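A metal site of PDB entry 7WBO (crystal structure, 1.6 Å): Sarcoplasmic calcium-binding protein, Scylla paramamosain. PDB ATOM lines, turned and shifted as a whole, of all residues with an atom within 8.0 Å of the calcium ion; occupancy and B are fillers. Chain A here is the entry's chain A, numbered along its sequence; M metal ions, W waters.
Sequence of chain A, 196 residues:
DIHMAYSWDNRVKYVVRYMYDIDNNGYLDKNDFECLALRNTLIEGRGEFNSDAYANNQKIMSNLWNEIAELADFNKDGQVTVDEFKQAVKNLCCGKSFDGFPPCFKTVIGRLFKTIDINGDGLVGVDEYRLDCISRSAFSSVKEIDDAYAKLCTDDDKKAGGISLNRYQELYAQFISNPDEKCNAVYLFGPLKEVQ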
ATOM      1  N   VAL A  16      17.897 -28.460  -4.584  1.00  0.00           N
ATOM      2  CA  VAL A  16      18.760 -27.358  -5.067  1.00  0.00           C
ATOM      3  C   VAL A  16      19.129 -26.492  -3.865  1.00  0.00           C
ATOM      4  O   VAL A  16      20.307 -26.157  -3.713  1.00  0.00           O
ATOM      5  CB  VAL A  16      18.061 -26.534  -6.148  1.00  0.00           C
ATOM      6  CG1 VAL A  16      18.906 -25.328  -6.508  1.00  0.00           C
ATOM      7  CG2 VAL A  16      17.740 -27.403  -7.327  1.00  0.00           C
ATOM      8  N   ARG A  17      18.163 -26.147  -3.037  1.00  0.00           N
ATOM      9  CA  ARG A  17      18.389 -25.250  -1.875  1.00  0.00           C
ATOM     10  C   ARG A  17      19.426 -25.870  -0.943  1.00  0.00           C
ATOM     11  O   ARG A  17      20.428 -25.166  -0.571  1.00  0.00           O
ATOM     12  CB  ARG A  17      17.073 -24.996  -1.139  1.00  0.00           C
ATOM     13  CG  ARG A  17      17.226 -24.234   0.188  1.00  0.00           C
ATOM     14  CD  ARG A  17      17.638 -22.782   0.092  1.00  0.00           C
ATOM     15  NE  ARG A  17      16.716 -21.958  -0.692  1.00  0.00           N
ATOM     16  CZ  ARG A  17      15.516 -21.487  -0.304  1.00  0.00           C
ATOM     17  NH1 ARG A  17      14.803 -20.772  -1.170  1.00  0.00           N
ATOM     18  NH2 ARG A  17      15.013 -21.718   0.904  1.00  0.00           N
ATOM     19  N   TYR A  20      22.895 -27.975  -2.724  1.00  0.00           N
ATOM     20  CA  TYR A  20      23.805 -27.291  -3.672  1.00  0.00           C
ATOM     21  C   TYR A  20      23.928 -25.788  -3.428  1.00  0.00           C
ATOM     22  O   TYR A  20      25.039 -25.261  -3.551  1.00  0.00           O
ATOM     23  CB  TYR A  20      23.384 -27.531  -5.123  1.00  0.00           C
ATOM     24  CG  TYR A  20      23.448 -28.964  -5.590  1.00  0.00           C
ATOM     25  CD1 TYR A  20      24.637 -29.541  -6.009  1.00  0.00           C
ATOM     26  CD2 TYR A  20      22.318 -29.754  -5.603  1.00  0.00           C
ATOM     27  CE1 TYR A  20      24.656 -30.837  -6.480  1.00  0.00           C
ATOM     28  CE2 TYR A  20      22.328 -31.074  -6.015  1.00  0.00           C
ATOM     29  CZ  TYR A  20      23.510 -31.622  -6.469  1.00  0.00           C
ATOM     30  OH  TYR A  20      23.567 -32.928  -6.895  1.00  0.00           O
ATOM     31  N   ASP A  21      22.834 -25.094  -3.123  1.00  0.00           N
ATOM     32  CA  ASP A  21      22.822 -23.610  -3.057  1.00  0.00           C
ATOM     33  C   ASP A  21      23.375 -23.165  -1.703  1.00  0.00           C
ATOM     34  O   ASP A  21      22.672 -22.495  -0.976  1.00  0.00           O
ATOM     35  CB  ASP A  21      21.418 -23.040  -3.306  1.00  0.00           C
ATOM     36  CG  ASP A  21      21.395 -21.528  -3.416  1.00  0.00           C
ATOM     37  OD1 ASP A  21      22.472 -20.899  -3.605  1.00  0.00           O
ATOM     38  OD2 ASP A  21      20.320 -20.934  -3.250  1.00  0.00           O
ATOM     39  N   ILE A  22      24.660 -23.448  -1.455  1.00  0.00           N
ATOM     40  CA  ILE A  22      25.234 -23.230  -0.088  1.00  0.00           C
ATOM     41  C   ILE A  22      25.227 -21.732   0.259  1.00  0.00           C
ATOM     42  O   ILE A  22      25.088 -21.401   1.491  1.00  0.00           O
ATOM     43  CB  ILE A  22      26.624 -23.853  -0.001  1.00  0.00           C
ATOM     44  CG1 ILE A  22      27.101 -23.848   1.452  1.00  0.00           C
ATOM     45  CG2 ILE A  22      27.581 -23.127  -0.883  1.00  0.00           C
ATOM     46  CD1 ILE A  22      28.492 -24.367   1.623  1.00  0.00           C
ATOM     47  N   ASP A  23      25.395 -20.816  -0.710  1.00  0.00           N
ATOM     48  CA  ASP A  23      25.430 -19.374  -0.385  1.00  0.00           C
ATOM     49  C   ASP A  23      24.031 -18.755  -0.366  1.00  0.00           C
ATOM     50  O   ASP A  23      23.919 -17.543  -0.129  1.00  0.00           O
ATOM     51  CB  ASP A  23      26.442 -18.652  -1.256  1.00  0.00           C
ATOM     52  CG  ASP A  23      26.040 -18.489  -2.707  1.00  0.00           C
ATOM     53  OD1 ASP A  23      24.887 -18.762  -3.050  1.00  0.00           O
ATOM     54  OD2 ASP A  23      26.949 -18.102  -3.509  1.00  0.00           O
ATOM     55  N   ASN A  24      22.988 -19.579  -0.589  1.00  0.00           N
ATOM     56  CA  ASN A  24      21.561 -19.254  -0.347  1.00  0.00           C
ATOM     57  C   ASN A  24      21.172 -18.027  -1.147  1.00  0.00           C
ATOM     58  O   ASN A  24      20.416 -17.182  -0.632  1.00  0.00           O
ATOM     59  CB  ASN A  24      21.275 -19.069   1.165  1.00  0.00           C
ATOM     60  CG  ASN A  24      19.791 -19.031   1.446  1.00  0.00           C
ATOM     61  OD1 ASN A  24      19.014 -19.739   0.830  1.00  0.00           O
ATOM     62  ND2 ASN A  24      19.365 -18.141   2.322  1.00  0.00           N
ATOM     63  N   ASN A  25      21.607 -17.904  -2.405  1.00  0.00           N
ATOM     64  CA  ASN A  25      21.161 -16.763  -3.260  1.00  0.00           C
ATOM     65  C   ASN A  25      20.136 -17.195  -4.319  1.00  0.00           C
ATOM     66  O   ASN A  25      19.741 -16.337  -5.107  1.00  0.00           O
ATOM     67  CB  ASN A  25      22.319 -16.034  -3.918  1.00  0.00           C
ATOM     68  CG  ASN A  25      23.111 -16.894  -4.886  1.00  0.00           C
ATOM     69  OD1 ASN A  25      22.812 -18.055  -5.092  1.00  0.00           O
ATOM     70  ND2 ASN A  25      24.193 -16.360  -5.396  1.00  0.00           N
ATOM     71  N   GLY A  26      19.667 -18.439  -4.280  1.00  0.00           N
ATOM     72  CA  GLY A  26      18.521 -18.886  -5.098  1.00  0.00           C
ATOM     73  C   GLY A  26      18.940 -19.585  -6.381  1.00  0.00           C
ATOM     74  O   GLY A  26      18.069 -20.125  -7.046  1.00  0.00           O
ATOM     75  N   TYR A  27      20.213 -19.545  -6.745  1.00  0.00           N
ATOM     76  CA  TYR A  27      20.702 -20.231  -7.967  1.00  0.00           C
ATOM     77  C   TYR A  27      22.071 -20.842  -7.733  1.00  0.00           C
ATOM     78  O   TYR A  27      22.730 -20.532  -6.729  1.00  0.00           O
ATOM     79  CB  TYR A  27      20.771 -19.279  -9.161  1.00  0.00           C
ATOM     80  CG  TYR A  27      21.673 -18.072  -8.988  1.00  0.00           C
ATOM     81  CD1 TYR A  27      23.021 -18.170  -9.236  1.00  0.00           C
ATOM     82  CD2 TYR A  27      21.188 -16.888  -8.442  1.00  0.00           C
ATOM     83  CE1 TYR A  27      23.897 -17.113  -8.994  1.00  0.00           C
ATOM     84  CE2 TYR A  27      22.051 -15.808  -8.255  1.00  0.00           C
ATOM     85  CZ  TYR A  27      23.389 -15.929  -8.523  1.00  0.00           C
ATOM     86  OH  TYR A  27      24.265 -14.885  -8.321  1.00  0.00           O
ATOM     87  N   LEU A  28      22.536 -21.688  -8.635  1.00  0.00           N
ATOM     88  CA  LEU A  28      23.838 -22.380  -8.498  1.00  0.00           C
ATOM     89  C   LEU A  28      24.869 -21.680  -9.379  1.00  0.00           C
ATOM     90  O   LEU A  28      24.547 -21.334 -10.547  1.00  0.00           O
ATOM     91  CB  LEU A  28      23.731 -23.854  -8.907  1.00  0.00           C
ATOM     92  CG  LEU A  28      22.646 -24.622  -8.160  1.00  0.00           C
ATOM     93  CD1 LEU A  28      22.664 -26.078  -8.542  1.00  0.00           C
ATOM     94  CD2 LEU A  28      22.735 -24.370  -6.680  1.00  0.00           C
ATOM     95  N   ASP A  29      26.064 -21.457  -8.846  1.00  0.00           N
ATOM     96  CA  ASP A  29      27.197 -21.053  -9.717  1.00  0.00           C
ATOM     97  C   ASP A  29      28.484 -21.512  -9.036  1.00  0.00           C
ATOM     98  O   ASP A  29      28.410 -22.185  -8.049  1.00  0.00           O
ATOM     99  CB  ASP A  29      27.176 -19.558 -10.018  1.00  0.00           C
ATOM    100  CG  ASP A  29      27.539 -18.635  -8.874  1.00  0.00           C
ATOM    101  OD1 ASP A  29      27.805 -19.115  -7.786  1.00  0.00           O
ATOM    102  OD2 ASP A  29      27.606 -17.419  -9.127  1.00  0.00           O
ATOM    103  N   LYS A  30      29.607 -21.104  -9.564  1.00  0.00           N
ATOM    104  CA  LYS A  30      30.900 -21.611  -9.100  1.00  0.00           C
ATOM    105  C   LYS A  30      31.101 -21.305  -7.634  1.00  0.00           C
ATOM    106  O   LYS A  30      31.662 -22.178  -6.974  1.00  0.00           O
ATOM    107  CB  LYS A  30      32.026 -20.954  -9.903  1.00  0.00           C
ATOM    108  CG  LYS A  30      33.340 -21.661  -9.679  1.00  0.00           C
ATOM    109  CD  LYS A  30      34.420 -21.221 -10.626  1.00  0.00           C
ATOM    110  CE  LYS A  30      34.918 -19.838 -10.279  1.00  0.00           C
ATOM    111  NZ  LYS A  30      33.857 -18.822 -10.410  1.00  0.00           N
ATOM    112  N   ASN A  31      30.597 -20.174  -7.159  1.00  0.00           N
ATOM    113  CA  ASN A  31      30.821 -19.803  -5.733  1.00  0.00           C
ATOM    114  C   ASN A  31      30.206 -20.889  -4.835  1.00  0.00           C
ATOM    115  O   ASN A  31      30.773 -21.200  -3.779  1.00  0.00           O
ATOM    116  CB  ASN A  31      30.208 -18.459  -5.393  1.00  0.00           C
ATOM    117  CG  ASN A  31      30.664 -18.018  -4.015  1.00  0.00           C
ATOM    118  OD1 ASN A  31      31.876 -17.932  -3.771  1.00  0.00           O
ATOM    119  ND2 ASN A  31      29.742 -17.831  -3.105  1.00  0.00           N
ATOM    120  N   ASP A  32      29.053 -21.469  -5.191  1.00  0.00           N
ATOM    121  CA  ASP A  32      28.468 -22.528  -4.331  1.00  0.00           C
ATOM    122  C   ASP A  32      29.473 -23.666  -4.137  1.00  0.00           C
ATOM    123  O   ASP A  32      29.644 -24.214  -3.013  1.00  0.00           O
ATOM    124  CB  ASP A  32      27.164 -23.072  -4.894  1.00  0.00           C
ATOM    125  CG  ASP A  32      26.072 -22.034  -4.836  1.00  0.00           C
ATOM    126  OD1 ASP A  32      25.750 -21.512  -3.766  1.00  0.00           O
ATOM    127  OD2 ASP A  32      25.503 -21.748  -5.924  1.00  0.00           O
ATOM    128  N   PHE A  33      30.118 -24.050  -5.226  1.00  0.00           N
ATOM    129  CA  PHE A  33      30.999 -25.228  -5.233  1.00  0.00           C
ATOM    130  C   PHE A  33      32.315 -24.879  -4.542  1.00  0.00           C
ATOM    131  O   PHE A  33      32.776 -25.779  -3.866  1.00  0.00           O
ATOM    132  CB  PHE A  33      31.048 -25.758  -6.659  1.00  0.00           C
ATOM    133  CG  PHE A  33      29.687 -26.304  -7.036  1.00  0.00           C
ATOM    134  CD1 PHE A  33      28.751 -25.444  -7.630  1.00  0.00           C
ATOM    135  CD2 PHE A  33      29.315 -27.595  -6.763  1.00  0.00           C
ATOM    136  CE1 PHE A  33      27.481 -25.897  -7.923  1.00  0.00           C
ATOM    137  CE2 PHE A  33      28.047 -28.044  -7.072  1.00  0.00           C
ATOM    138  CZ  PHE A  33      27.139 -27.189  -7.664  1.00  0.00           C
ATOM    139  N   VAL A  80      23.029 -21.912 -12.804  1.00  0.00           N
ATOM    140  CA  VAL A  80      21.945 -22.910 -13.013  1.00  0.00           C
ATOM    141  C   VAL A  80      20.813 -22.591 -12.050  1.00  0.00           C
ATOM    142  O   VAL A  80      21.003 -22.618 -10.804  1.00  0.00           O
ATOM    143  CB  VAL A  80      22.452 -24.359 -12.840  1.00  0.00           C
ATOM    144  CG1 VAL A  80      21.330 -25.367 -12.731  1.00  0.00           C
ATOM    145  CG2 VAL A  80      23.365 -24.750 -13.958  1.00  0.00           C
HETATM  146 CA    CA M   1      24.123 -19.997  -4.963  1.00  0.00          CA
HETATM  147  O   HOH W   1      25.951 -18.640  -5.878  1.00  0.00           O
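The calcium ion is bound by the backbone carbonyl oxygen (O) of Tyr 27 (2.3 Å), the side-chain carboxylate (OD1) of Asp 21 (2.3 Å), the side-chain amide oxygen (OD1) of Asn 25 (2.3 Å), the side-chain carboxylate (OD1) of Asp 23 (2.4 Å), the side-chain carboxylate (OD2) of Asp 32 (2.4 Å), water W1 (2.5 Å) and the side-chain carboxylate (OD1) of Asp 32 (2.5 Å).
N of Asn 24 lies close to OD1 of Asp 21.
The backbone NH (N) of Gly 26 lies within hydrogen-bond range of the side-chain carboxylate (OD2) of Asp 21 (2.8 Å).
N of Asp 21 sits at hydrogen-bond distance from O of Val 16, at 2.8 Å.
OD2 of Asp 23 is in hydrogen-bond range of ND2 of Asn 31.
The backbone NH (N) of Asp 29 sits close to the side-chain carboxylate (OD2) of Asp 32, 3.0 Å away.
The backbone NH (N) of Ile 22 lies close to the side-chain carboxylate (OD1) of Asp 32, 3.2 Å away.
Water W1 lies within hydrogen-bond range of OD2 of Asp 23 (2.6 Å), OD1 of Asp 29 (2.7 Å) and ND2 of Asn 25 (2.9 Å).
Along chain A the residues within 4 Å of the calcium ion span positions 21 to 32.
The nearest printed residue that does not touch the calcium ion is Leu 28 (4.3 Å).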
